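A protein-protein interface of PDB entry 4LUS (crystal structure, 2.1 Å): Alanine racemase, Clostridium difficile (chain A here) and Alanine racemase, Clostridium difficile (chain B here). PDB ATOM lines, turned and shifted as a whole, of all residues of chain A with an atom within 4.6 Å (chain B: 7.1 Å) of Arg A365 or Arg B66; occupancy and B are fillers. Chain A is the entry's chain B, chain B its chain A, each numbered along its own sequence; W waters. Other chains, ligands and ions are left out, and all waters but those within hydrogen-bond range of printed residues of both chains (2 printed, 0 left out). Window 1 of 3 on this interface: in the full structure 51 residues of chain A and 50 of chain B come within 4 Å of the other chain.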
ATOM      1  N   PRO A   7       0.686 -18.298 -29.053  1.00  0.00           N
ATOM      2  CA  PRO A   7      -0.466 -17.827 -28.301  1.00  0.00           C
ATOM      3  C   PRO A   7      -0.178 -16.930 -27.130  1.00  0.00           C
ATOM      4  O   PRO A   7      -1.067 -16.320 -26.648  1.00  0.00           O
ATOM      5  CB  PRO A   7      -1.076 -19.096 -27.797  1.00  0.00           C
ATOM      6  CG  PRO A   7       0.047 -19.992 -27.637  1.00  0.00           C
ATOM      7  CD  PRO A   7       0.989 -19.691 -28.730  1.00  0.00           C
ATOM      8  N   PRO A 284      -4.427 -19.362 -22.763  1.00  0.00           N
ATOM      9  CA  PRO A 284      -3.306 -20.294 -22.870  1.00  0.00           C
ATOM     10  C   PRO A 284      -1.966 -19.734 -22.322  1.00  0.00           C
ATOM     11  O   PRO A 284      -0.992 -19.634 -22.994  1.00  0.00           O
ATOM     12  CB  PRO A 284      -3.239 -20.590 -24.362  1.00  0.00           C
ATOM     13  CG  PRO A 284      -3.682 -19.355 -24.994  1.00  0.00           C
ATOM     14  CD  PRO A 284      -4.641 -18.689 -24.038  1.00  0.00           C
ATOM     15  N   ILE A 285      -1.991 -19.394 -21.059  1.00  0.00           N
ATOM     16  CA  ILE A 285      -0.811 -19.095 -20.266  1.00  0.00           C
ATOM     17  C   ILE A 285      -0.900 -19.789 -18.915  1.00  0.00           C
ATOM     18  O   ILE A 285      -1.956 -19.902 -18.368  1.00  0.00           O
ATOM     19  CB  ILE A 285      -0.569 -17.586 -20.105  1.00  0.00           C
ATOM     20  CG1 ILE A 285       0.848 -17.275 -19.603  1.00  0.00           C
ATOM     21  CG2 ILE A 285      -1.560 -16.947 -19.178  1.00  0.00           C
ATOM     22  CD1 ILE A 285       1.216 -15.840 -19.615  1.00  0.00           C
ATOM     23  N   GLY A 286       0.236 -20.225 -18.407  1.00  0.00           N
ATOM     24  CA  GLY A 286       0.380 -20.992 -17.202  1.00  0.00           C
ATOM     25  C   GLY A 286       1.671 -20.728 -16.436  1.00  0.00           C
ATOM     26  O   GLY A 286       2.430 -19.869 -16.790  1.00  0.00           O
ATOM     27  N   ALA A 288       4.270 -22.583 -16.357  1.00  0.00           N
ATOM     28  CA  ALA A 288       5.415 -22.832 -17.200  1.00  0.00           C
ATOM     29  C   ALA A 288       5.816 -21.634 -18.062  1.00  0.00           C
ATOM     30  O   ALA A 288       6.876 -21.595 -18.514  1.00  0.00           O
ATOM     31  CB  ALA A 288       5.310 -24.126 -17.967  1.00  0.00           C
ATOM     32  N   ASP A 289       4.942 -20.660 -18.213  1.00  0.00           N
ATOM     33  CA  ASP A 289       5.250 -19.406 -18.843  1.00  0.00           C
ATOM     34  C   ASP A 289       5.868 -18.343 -17.914  1.00  0.00           C
ATOM     35  O   ASP A 289       6.333 -17.334 -18.340  1.00  0.00           O
ATOM     36  CB  ASP A 289       4.049 -18.869 -19.582  1.00  0.00           C
ATOM     37  CG  ASP A 289       3.494 -19.836 -20.566  1.00  0.00           C
ATOM     38  OD1 ASP A 289       4.101 -20.053 -21.562  1.00  0.00           O
ATOM     39  OD2 ASP A 289       2.458 -20.373 -20.344  1.00  0.00           O
ATOM     40  N   MET A 315      -0.188 -25.542 -15.674  1.00  0.00           N
ATOM     41  CA  MET A 315       1.120 -25.384 -16.283  1.00  0.00           C
ATOM     42  C   MET A 315       1.077 -24.499 -17.535  1.00  0.00           C
ATOM     43  O   MET A 315       1.929 -23.732 -17.740  1.00  0.00           O
ATOM     44  CB  MET A 315       1.705 -26.752 -16.649  1.00  0.00           C
ATOM     45  CG  MET A 315       3.108 -26.855 -17.207  1.00  0.00           C
ATOM     46  SD  MET A 315       3.628 -28.515 -17.585  1.00  0.00           S
ATOM     47  CE  MET A 315       3.989 -29.145 -16.017  1.00  0.00           C
ATOM     48  N   ASP A 316       0.069 -24.691 -18.351  1.00  0.00           N
ATOM     49  CA  ASP A 316      -0.068 -24.007 -19.622  1.00  0.00           C
ATOM     50  C   ASP A 316      -1.315 -23.166 -19.816  1.00  0.00           C
ATOM     51  O   ASP A 316      -1.456 -22.522 -20.787  1.00  0.00           O
ATOM     52  CB  ASP A 316       0.080 -24.996 -20.791  1.00  0.00           C
ATOM     53  CG  ASP A 316       1.004 -26.115 -20.478  1.00  0.00           C
ATOM     54  OD1 ASP A 316       2.145 -25.842 -20.374  1.00  0.00           O
ATOM     55  OD2 ASP A 316       0.566 -27.211 -20.291  1.00  0.00           O
ATOM     56  N   SER A 363       9.263 -17.310 -19.345  1.00  0.00           N
ATOM     57  CA  SER A 363       9.981 -18.487 -19.735  1.00  0.00           C
ATOM     58  C   SER A 363      10.499 -18.322 -21.107  1.00  0.00           C
ATOM     59  O   SER A 363      10.042 -17.521 -21.850  1.00  0.00           O
ATOM     60  CB  SER A 363       9.059 -19.655 -19.726  1.00  0.00           C
ATOM     61  OG  SER A 363       8.899 -19.926 -18.439  1.00  0.00           O
ATOM     62  N   ARG A 364      11.195 -19.408 -21.486  1.00  0.00           N
ATOM     63  CA  ARG A 364      11.934 -19.659 -22.689  1.00  0.00           C
ATOM     64  C   ARG A 364      10.955 -19.685 -23.867  1.00  0.00           C
ATOM     65  O   ARG A 364      11.193 -19.101 -24.845  1.00  0.00           O
ATOM     66  CB  ARG A 364      12.777 -20.949 -22.642  1.00  0.00           C
ATOM     67  CG  ARG A 364      13.555 -21.189 -23.911  1.00  0.00           C
ATOM     68  CD  ARG A 364      14.445 -22.415 -24.043  1.00  0.00           C
ATOM     69  NE  ARG A 364      13.601 -23.552 -24.223  1.00  0.00           N
ATOM     70  CZ  ARG A 364      13.612 -24.380 -25.223  1.00  0.00           C
ATOM     71  NH1 ARG A 364      14.468 -24.321 -26.171  1.00  0.00           N
ATOM     72  NH2 ARG A 364      12.734 -25.312 -25.210  1.00  0.00           N
ATOM     73  N   ARG A 365       9.834 -20.335 -23.663  1.00  0.00           N
ATOM     74  CA  ARG A 365       8.838 -20.506 -24.658  1.00  0.00           C
ATOM     75  C   ARG A 365       8.055 -19.258 -24.894  1.00  0.00           C
ATOM     76  O   ARG A 365       7.306 -19.241 -25.781  1.00  0.00           O
ATOM     77  CB  ARG A 365       7.942 -21.706 -24.413  1.00  0.00           C
ATOM     78  CG  ARG A 365       6.932 -21.587 -23.299  1.00  0.00           C
ATOM     79  CD  ARG A 365       6.035 -22.795 -23.225  1.00  0.00           C
ATOM     80  NE  ARG A 365       4.965 -22.640 -22.285  1.00  0.00           N
ATOM     81  CZ  ARG A 365       4.299 -23.608 -21.714  1.00  0.00           C
ATOM     82  NH1 ARG A 365       4.556 -24.864 -21.998  1.00  0.00           N
ATOM     83  NH2 ARG A 365       3.366 -23.315 -20.852  1.00  0.00           N
ATOM     84  N   VAL A 366       8.251 -18.226 -24.114  1.00  0.00           N
ATOM     85  CA  VAL A 366       7.530 -16.988 -24.352  1.00  0.00           C
ATOM     86  C   VAL A 366       8.291 -16.088 -25.341  1.00  0.00           C
ATOM     87  O   VAL A 366       9.223 -15.498 -25.003  1.00  0.00           O
ATOM     88  CB  VAL A 366       7.185 -16.255 -23.056  1.00  0.00           C
ATOM     89  CG1 VAL A 366       6.362 -15.022 -23.308  1.00  0.00           C
ATOM     90  CG2 VAL A 366       6.483 -17.158 -22.074  1.00  0.00           C
ATOM     91  N   ASP A 367       7.837 -16.032 -26.574  1.00  0.00           N
ATOM     92  CA  ASP A 367       8.510 -15.300 -27.608  1.00  0.00           C
ATOM     93  C   ASP A 367       8.582 -13.831 -27.197  1.00  0.00           C
ATOM     94  O   ASP A 367       7.672 -13.316 -26.665  1.00  0.00           O
ATOM     95  CB  ASP A 367       7.727 -15.382 -28.906  1.00  0.00           C
ATOM     96  CG  ASP A 367       7.944 -16.652 -29.680  1.00  0.00           C
ATOM     97  OD1 ASP A 367       8.365 -17.665 -29.179  1.00  0.00           O
ATOM     98  OD2 ASP A 367       7.666 -16.600 -30.847  1.00  0.00           O
ATOM     99  N   LEU A 383      12.763 -21.213 -29.121  1.00  0.00           N
ATOM    100  CA  LEU A 383      12.613 -22.617 -29.435  1.00  0.00           C
ATOM    101  C   LEU A 383      13.009 -22.974 -30.870  1.00  0.00           C
ATOM    102  O   LEU A 383      13.517 -23.991 -31.134  1.00  0.00           O
ATOM    103  CB  LEU A 383      11.198 -23.050 -29.181  1.00  0.00           C
ATOM    104  CG  LEU A 383      10.751 -23.512 -27.808  1.00  0.00           C
ATOM    105  CD1 LEU A 383      10.994 -22.513 -26.713  1.00  0.00           C
ATOM    106  CD2 LEU A 383       9.322 -23.988 -27.826  1.00  0.00           C
ATOM    107  N1  LLP B  39      -2.853 -34.760 -20.117  1.00  0.00           N
ATOM    108  C2  LLP B  39      -3.193 -33.521 -20.185  1.00  0.00           C
ATOM    109  C2' LLP B  39      -4.380 -33.118 -20.973  1.00  0.00           C
ATOM    110  C3  LLP B  39      -2.392 -32.514 -19.481  1.00  0.00           C
ATOM    111  O3  LLP B  39      -2.649 -31.247 -19.526  1.00  0.00           O
ATOM    112  C4  LLP B  39      -1.231 -32.940 -18.755  1.00  0.00           C
ATOM    113  C4' LLP B  39      -0.385 -31.918 -18.057  1.00  0.00           C
ATOM    114  C5  LLP B  39      -0.969 -34.371 -18.744  1.00  0.00           C
ATOM    115  C6  LLP B  39      -1.820 -35.177 -19.434  1.00  0.00           C
ATOM    116  C5' LLP B  39       0.167 -34.945 -17.980  1.00  0.00           C
ATOM    117  OP4 LLP B  39      -0.072 -34.709 -16.618  1.00  0.00           O
ATOM    118  P   LLP B  39       0.573 -35.419 -15.423  1.00  0.00           P
ATOM    119  OP1 LLP B  39       0.009 -34.934 -14.266  1.00  0.00           O
ATOM    120  OP2 LLP B  39       0.472 -36.802 -15.597  1.00  0.00           O
ATOM    121  OP3 LLP B  39       1.921 -35.017 -15.416  1.00  0.00           O
ATOM    122  N   LLP B  39       5.491 -31.436 -22.585  1.00  0.00           N
ATOM    123  CA  LLP B  39       5.201 -30.046 -22.615  1.00  0.00           C
ATOM    124  CB  LLP B  39       3.726 -29.844 -22.346  1.00  0.00           C
ATOM    125  CG  LLP B  39       3.296 -30.050 -20.920  1.00  0.00           C
ATOM    126  CD  LLP B  39       1.853 -30.483 -20.845  1.00  0.00           C
ATOM    127  CE  LLP B  39       1.527 -31.085 -19.489  1.00  0.00           C
ATOM    128  NZ  LLP B  39       0.167 -30.983 -19.014  1.00  0.00           N
ATOM    129  C   LLP B  39       6.117 -29.288 -21.673  1.00  0.00           C
ATOM    130  O   LLP B  39       6.712 -29.869 -20.824  1.00  0.00           O
ATOM    131  N   ALA B  40       6.236 -28.006 -21.875  1.00  0.00           N
ATOM    132  CA  ALA B  40       7.053 -27.172 -21.054  1.00  0.00           C
ATOM    133  C   ALA B  40       8.493 -27.643 -21.026  1.00  0.00           C
ATOM    134  O   ALA B  40       9.119 -27.697 -20.018  1.00  0.00           O
ATOM    135  CB  ALA B  40       6.492 -27.057 -19.662  1.00  0.00           C
ATOM    136  N   ASP B  41       8.971 -27.943 -22.209  1.00  0.00           N
ATOM    137  CA  ASP B  41      10.322 -28.387 -22.428  1.00  0.00           C
ATOM    138  C   ASP B  41      10.594 -29.636 -21.620  1.00  0.00           C
ATOM    139  O   ASP B  41      11.489 -29.678 -20.879  1.00  0.00           O
ATOM    140  CB  ASP B  41      11.331 -27.245 -22.147  1.00  0.00           C
ATOM    141  CG  ASP B  41      12.738 -27.572 -22.579  1.00  0.00           C
ATOM    142  OD1 ASP B  41      12.855 -28.214 -23.571  1.00  0.00           O
ATOM    143  OD2 ASP B  41      13.682 -27.171 -21.922  1.00  0.00           O
ATOM    144  N   ALA B  63       3.207 -35.645 -26.457  1.00  0.00           N
ATOM    145  CA  ALA B  63       2.313 -34.557 -26.248  1.00  0.00           C
ATOM    146  C   ALA B  63       2.982 -33.273 -25.835  1.00  0.00           C
ATOM    147  O   ALA B  63       3.813 -33.255 -25.009  1.00  0.00           O
ATOM    148  CB  ALA B  63       1.221 -34.934 -25.301  1.00  0.00           C
ATOM    149  N   VAL B  64       2.554 -32.199 -26.442  1.00  0.00           N
ATOM    150  CA  VAL B  64       3.027 -30.864 -26.191  1.00  0.00           C
ATOM    151  C   VAL B  64       1.915 -29.924 -25.766  1.00  0.00           C
ATOM    152  O   VAL B  64       0.824 -30.282 -25.784  1.00  0.00           O
ATOM    153  CB  VAL B  64       3.760 -30.257 -27.394  1.00  0.00           C
ATOM    154  CG1 VAL B  64       5.021 -30.995 -27.670  1.00  0.00           C
ATOM    155  CG2 VAL B  64       2.862 -30.123 -28.592  1.00  0.00           C
ATOM    156  N   ALA B  65       2.251 -28.735 -25.348  1.00  0.00           N
ATOM    157  CA  ALA B  65       1.262 -27.734 -25.043  1.00  0.00           C
ATOM    158  C   ALA B  65       1.122 -26.607 -26.045  1.00  0.00           C
ATOM    159  O   ALA B  65       0.238 -25.878 -25.958  1.00  0.00           O
ATOM    160  CB  ALA B  65       1.460 -27.164 -23.660  1.00  0.00           C
ATOM    161  N   ARG B  66       2.038 -26.485 -26.964  1.00  0.00           N
ATOM    162  CA  ARG B  66       2.067 -25.387 -27.882  1.00  0.00           C
ATOM    163  C   ARG B  66       2.550 -25.850 -29.216  1.00  0.00           C
ATOM    164  O   ARG B  66       3.282 -26.773 -29.310  1.00  0.00           O
ATOM    165  CB  ARG B  66       2.985 -24.308 -27.351  1.00  0.00           C
ATOM    166  CG  ARG B  66       2.675 -23.800 -25.983  1.00  0.00           C
ATOM    167  CD  ARG B  66       1.545 -22.787 -25.941  1.00  0.00           C
ATOM    168  NE  ARG B  66       1.555 -22.158 -24.683  1.00  0.00           N
ATOM    169  CZ  ARG B  66       0.680 -22.341 -23.725  1.00  0.00           C
ATOM    170  NH1 ARG B  66      -0.369 -23.078 -23.912  1.00  0.00           N
ATOM    171  NH2 ARG B  66       0.887 -21.758 -22.582  1.00  0.00           N
ATOM    172  N   THR B  67       2.162 -25.164 -30.249  1.00  0.00           N
ATOM    173  CA  THR B  67       2.544 -25.540 -31.571  1.00  0.00           C
ATOM    174  C   THR B  67       4.042 -25.499 -31.698  1.00  0.00           C
ATOM    175  O   THR B  67       4.622 -26.394 -32.184  1.00  0.00           O
ATOM    176  CB  THR B  67       2.020 -24.579 -32.614  1.00  0.00           C
ATOM    177  OG1 THR B  67       0.654 -24.341 -32.422  1.00  0.00           O
ATOM    178  CG2 THR B  67       2.261 -25.126 -33.943  1.00  0.00           C
ATOM    179  N   ALA B  68       4.631 -24.449 -31.174  1.00  0.00           N
ATOM    180  CA  ALA B  68       6.027 -24.229 -31.241  1.00  0.00           C
ATOM    181  C   ALA B  68       6.833 -25.321 -30.585  1.00  0.00           C
ATOM    182  O   ALA B  68       7.892 -25.588 -30.998  1.00  0.00           O
ATOM    183  CB  ALA B  68       6.356 -22.899 -30.680  1.00  0.00           C
ATOM    184  N   GLU B  69       6.295 -25.901 -29.544  1.00  0.00           N
ATOM    185  CA  GLU B  69       6.875 -27.039 -28.906  1.00  0.00           C
ATOM    186  C   GLU B  69       6.918 -28.237 -29.847  1.00  0.00           C
ATOM    187  O   GLU B  69       7.901 -28.901 -29.917  1.00  0.00           O
ATOM    188  CB  GLU B  69       6.191 -27.376 -27.585  1.00  0.00           C
ATOM    189  CG  GLU B  69       6.596 -26.501 -26.421  1.00  0.00           C
ATOM    190  CD  GLU B  69       5.835 -26.760 -25.129  1.00  0.00           C
ATOM    191  OE1 GLU B  69       4.874 -27.493 -25.132  1.00  0.00           O
ATOM    192  OE2 GLU B  69       6.236 -26.220 -24.116  1.00  0.00           O
ATOM    193  N   GLY B  70       5.844 -28.457 -30.582  1.00  0.00           N
ATOM    194  CA  GLY B  70       5.855 -29.433 -31.629  1.00  0.00           C
ATOM    195  C   GLY B  70       6.837 -29.170 -32.759  1.00  0.00           C
ATOM    196  O   GLY B  70       7.573 -30.027 -33.127  1.00  0.00           O
ATOM    197  N   ILE B  71       6.900 -27.954 -33.237  1.00  0.00           N
ATOM    198  CA  ILE B  71       7.806 -27.599 -34.283  1.00  0.00           C
ATOM    199  C   ILE B  71       9.271 -27.798 -33.906  1.00  0.00           C
ATOM    200  O   ILE B  71      10.003 -28.320 -34.690  1.00  0.00           O
ATOM    201  CB  ILE B  71       7.517 -26.232 -34.860  1.00  0.00           C
ATOM    202  CG1 ILE B  71       6.140 -26.229 -35.441  1.00  0.00           C
ATOM    203  CG2 ILE B  71       8.469 -25.893 -35.979  1.00  0.00           C
ATOM    204  CD1 ILE B  71       5.666 -24.873 -35.718  1.00  0.00           C
ATOM    205  N   ILE B  82       2.863 -36.275 -32.740  1.00  0.00           N
ATOM    206  CA  ILE B  82       2.826 -35.285 -31.733  1.00  0.00           C
ATOM    207  C   ILE B  82       1.449 -34.697 -31.595  1.00  0.00           C
ATOM    208  O   ILE B  82       0.910 -34.259 -32.532  1.00  0.00           O
ATOM    209  CB  ILE B  82       3.830 -34.170 -32.044  1.00  0.00           C
ATOM    210  CG1 ILE B  82       5.205 -34.750 -32.325  1.00  0.00           C
ATOM    211  CG2 ILE B  82       3.792 -33.099 -31.001  1.00  0.00           C
ATOM    212  CD1 ILE B  82       6.207 -33.767 -32.790  1.00  0.00           C
ATOM    213  N   LEU B  83       0.945 -34.670 -30.387  1.00  0.00           N
ATOM    214  CA  LEU B  83      -0.309 -34.054 -30.047  1.00  0.00           C
ATOM    215  C   LEU B  83      -0.177 -32.779 -29.237  1.00  0.00           C
ATOM    216  O   LEU B  83       0.453 -32.762 -28.220  1.00  0.00           O
ATOM    217  CB  LEU B  83      -1.197 -35.015 -29.293  1.00  0.00           C
ATOM    218  CG  LEU B  83      -2.475 -34.520 -28.615  1.00  0.00           C
ATOM    219  CD1 LEU B  83      -3.441 -34.041 -29.623  1.00  0.00           C
ATOM    220  CD2 LEU B  83      -3.116 -35.600 -27.758  1.00  0.00           C
ATOM    221  N   ASN B  84      -0.795 -31.728 -29.732  1.00  0.00           N
ATOM    222  CA  ASN B  84      -0.896 -30.481 -29.031  1.00  0.00           C
ATOM    223  C   ASN B  84      -2.166 -30.553 -28.223  1.00  0.00           C
ATOM    224  O   ASN B  84      -3.231 -30.574 -28.734  1.00  0.00           O
ATOM    225  CB  ASN B  84      -0.872 -29.266 -29.929  1.00  0.00           C
ATOM    226  CG  ASN B  84      -1.026 -27.950 -29.166  1.00  0.00           C
ATOM    227  OD1 ASN B  84      -1.206 -27.924 -27.986  1.00  0.00           O
ATOM    228  ND2 ASN B  84      -0.899 -26.876 -29.857  1.00  0.00           N
ATOM    229  N   LEU B  85      -1.951 -30.634 -26.930  1.00  0.00           N
ATOM    230  CA  LEU B  85      -2.987 -30.812 -25.931  1.00  0.00           C
ATOM    231  C   LEU B  85      -3.950 -29.688 -25.818  1.00  0.00           C
ATOM    232  O   LEU B  85      -4.993 -29.918 -25.494  1.00  0.00           O
ATOM    233  CB  LEU B  85      -2.448 -31.205 -24.576  1.00  0.00           C
ATOM    234  CG  LEU B  85      -1.607 -32.436 -24.441  1.00  0.00           C
ATOM    235  CD1 LEU B  85      -0.818 -32.341 -23.174  1.00  0.00           C
ATOM    236  CD2 LEU B  85      -2.380 -33.725 -24.524  1.00  0.00           C
ATOM    237  N   GLY B  86      -3.528 -28.479 -26.066  1.00  0.00           N
ATOM    238  CA  GLY B  86      -4.324 -27.303 -25.866  1.00  0.00           C
ATOM    239  C   GLY B  86      -4.685 -26.500 -27.075  1.00  0.00           C
ATOM    240  O   GLY B  86      -4.832 -27.019 -28.097  1.00  0.00           O
ATOM    241  N   TYR B  87      -4.807 -25.208 -26.896  1.00  0.00           N
ATOM    242  CA  TYR B  87      -5.237 -24.265 -27.908  1.00  0.00           C
ATOM    243  C   TYR B  87      -4.269 -24.117 -29.085  1.00  0.00           C
ATOM    244  O   TYR B  87      -3.115 -24.031 -28.921  1.00  0.00           O
ATOM    245  CB  TYR B  87      -5.567 -22.947 -27.216  1.00  0.00           C
ATOM    246  CG  TYR B  87      -5.787 -21.733 -28.043  1.00  0.00           C
ATOM    247  CD1 TYR B  87      -6.823 -21.640 -28.926  1.00  0.00           C
ATOM    248  CD2 TYR B  87      -4.978 -20.664 -27.910  1.00  0.00           C
ATOM    249  CE1 TYR B  87      -7.024 -20.521 -29.675  1.00  0.00           C
ATOM    250  CE2 TYR B  87      -5.161 -19.545 -28.668  1.00  0.00           C
ATOM    251  CZ  TYR B  87      -6.185 -19.475 -29.546  1.00  0.00           C
ATOM    252  OH  TYR B  87      -6.306 -18.343 -30.245  1.00  0.00           O
ATOM    253  N   THR B  88      -4.790 -24.157 -30.275  1.00  0.00           N
ATOM    254  CA  THR B  88      -4.067 -23.690 -31.404  1.00  0.00           C
ATOM    255  C   THR B  88      -4.778 -22.488 -31.981  1.00  0.00           C
ATOM    256  O   THR B  88      -5.854 -22.580 -32.435  1.00  0.00           O
ATOM    257  CB  THR B  88      -3.832 -24.772 -32.483  1.00  0.00           C
ATOM    258  OG1 THR B  88      -3.135 -25.877 -31.957  1.00  0.00           O
ATOM    259  CG2 THR B  88      -3.076 -24.224 -33.593  1.00  0.00           C
ATOM    260  N   SER B  96       0.933 -26.120 -38.179  1.00  0.00           N
ATOM    261  CA  SER B  96       0.605 -27.364 -37.567  1.00  0.00           C
ATOM    262  C   SER B  96       0.442 -28.482 -38.545  1.00  0.00           C
ATOM    263  O   SER B  96       0.930 -29.540 -38.327  1.00  0.00           O
ATOM    264  CB  SER B  96      -0.659 -27.259 -36.738  1.00  0.00           C
ATOM    265  OG  SER B  96      -0.403 -26.598 -35.587  1.00  0.00           O
ATOM    266  N   ILE B 101       1.631 -31.766 -36.627  1.00  0.00           N
ATOM    267  CA  ILE B 101       1.232 -31.572 -35.270  1.00  0.00           C
ATOM    268  C   ILE B 101      -0.273 -31.786 -35.218  1.00  0.00           C
ATOM    269  O   ILE B 101      -1.012 -31.031 -35.745  1.00  0.00           O
ATOM    270  CB  ILE B 101       1.640 -30.163 -34.757  1.00  0.00           C
ATOM    271  CG1 ILE B 101       3.139 -29.939 -34.810  1.00  0.00           C
ATOM    272  CG2 ILE B 101       1.207 -29.920 -33.348  1.00  0.00           C
ATOM    273  CD1 ILE B 101       3.961 -31.066 -34.332  1.00  0.00           C
ATOM    274  N   ARG B 364      16.534 -20.375 -18.712  1.00  0.00           N
ATOM    275  CA  ARG B 364      17.153 -20.550 -19.988  1.00  0.00           C
ATOM    276  C   ARG B 364      18.665 -20.609 -19.859  1.00  0.00           C
ATOM    277  O   ARG B 364      19.256 -21.356 -20.518  1.00  0.00           O
ATOM    278  CB  ARG B 364      16.747 -19.475 -21.007  1.00  0.00           C
ATOM    279  CG  ARG B 364      17.195 -19.751 -22.430  1.00  0.00           C
ATOM    280  CD  ARG B 364      16.713 -18.819 -23.550  1.00  0.00           C
ATOM    281  NE  ARG B 364      17.268 -17.597 -23.199  1.00  0.00           N
ATOM    282  CZ  ARG B 364      18.187 -16.921 -23.804  1.00  0.00           C
ATOM    283  NH1 ARG B 364      18.644 -17.218 -24.966  1.00  0.00           N
ATOM    284  NH2 ARG B 364      18.585 -15.878 -23.199  1.00  0.00           N
HETATM  285  O   HOH W   1       3.379 -20.023 -24.041  1.00  0.00           O
HETATM  286  O   HOH W   2       0.799 -30.224 -15.973  1.00  0.00           O
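Hydrophobic or aromatic side chains of chain B within 4 Å of the printed part of chain A: Ala B40, Ala B65 and Tyr B87.
Along chain B the printed residues that touch a printed residue of chain A span positions 39 to 364.
Of the 14 printed residues of chain A, 10 touch a printed residue of chain B.
Printed residues of chain A that touch a printed residue of chain B: Pro A7, Pro A284, Ile A285, Ala A288, Asp A289, Met A315, Asp A316, Arg A364, Arg A365 and Leu A383.
Hydrophobic or aromatic side chains of chain A within 4 Å of the printed part of chain B: Pro A7, Pro A284, Ala A288, Met A315 and Leu A383.
Among the printed residues, Asp or Glu carboxylates within 4 Å of a Lys or Arg side-chain nitrogen of the other chain: Asp A289 with Arg B66 (3.1 Å), Arg A364 with Asp B41 (3.3 Å) and Arg A365 with Glu B69 (3.0 Å).
The backbone carbonyl oxygen (O) of Ala B65 lies close to the side-chain amide oxygen (OD1) of Asn B84.
The backbone NH (N) of Gly A286 lies within hydrogen-bond range of the side-chain carboxylate (OD2) of Asp A289, at 3.0 Å.
The side-chain hydroxyl of Ser A363 lies within hydrogen-bond range of the backbone carbonyl oxygen of Ala A288.
NE of Arg A365 is in salt-bridge range of OD1 of Asp A289 (2.8 Å).
The guanidinium group (NH2) of Arg A365 is in hydrogen-bond range of the backbone carbonyl oxygen (O) of Met A315, at 3.5 Å.
OD1 of Asp A316 is in salt-bridge range of NH2 of Arg A365, at 2.8 Å.
Pro A7 touches Arg B66 (CG to CD, 3.6 Å).
Pro A284 touches Tyr B87 (CG to CD2, 3.4 Å).
Ile A285 touches Arg B66 (CA to NH2, 3.9 Å).
Ala A288 touches Ala B40.
Met A315 touches LLP B39 (SD to CG, 3.7 Å).
CD of LLP B39 touches OD2 of Asp A316, at 3.6 Å.
CG of Asp A316 touches CB of Ala B65, at 3.4 Å.
Arg B364 touches Arg A364.
Ala B40 touches Arg A365 (CA to NH1, 3.5 Å).
CG of Glu B69 touches CD2 of Leu A383, at 3.96 Å.
Of the printed residues of chain B, Met A315 touches LLP B39 (3.7 Å) and Ala B40 (3.8 Å).
Printed residues of chain B within 4 Å of Asp A316: LLP B39, Ala B65 and Arg B66.
Printed residues of chain B within 4 Å of Arg A364: Asp B41 and Arg B364.
Arg A365 touches just these residues of chain B: Ala B40, Arg B66 and Glu B69.
Of chain A, only Pro A7, Pro A284, Ile A285, Asp A289, Asp A316 and Arg A365 come within 4 Å of Arg B66.
Ile B71 touches none of the printed residues of chain A.
The nearest residue of chain B that does not touch Arg A365 is Ala B65 (4.2 Å).
The nearest residue of chain A that does not touch Arg B66 is Gly A286 (4.5 Å).
The nearest printed residue of chain A that does not touch Ala B68 is Asp A367 (5.8 Å).
The side-chain carboxylate of Asp B41 lies within salt-bridge range of the guanidinium group of Arg A364 (3.3 Å).
NH2 of Arg B66 lies within hydrogen-bond range of O of Pro A284, 2.9 Å away.
The side-chain carboxylate (OD2) of Asp A289 lies within salt-bridge range of the guanidinium group (NH2) of Arg B66, 3.1 Å away.
NH2 of Arg B66 lies within hydrogen-bond range of O of Asp A316.
NH1 of Arg A365 lies within salt-bridge range of OE2 of Glu B69, 3.0 Å away.
The guanidinium group (NH2) of Arg B66 sits close to the guanidinium group (NH2) of Arg A365 (3.4 Å).
Water W1 bridges the side-chain carboxylate (OD1) of Asp A289 (2.6 Å) and the guanidinium group (NE) of Arg B66 (2.9 Å).
Water W2 lies within hydrogen-bond range of NZ of LLP B39 (3.2 Å) and SD of Met A315 (3.7 Å).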
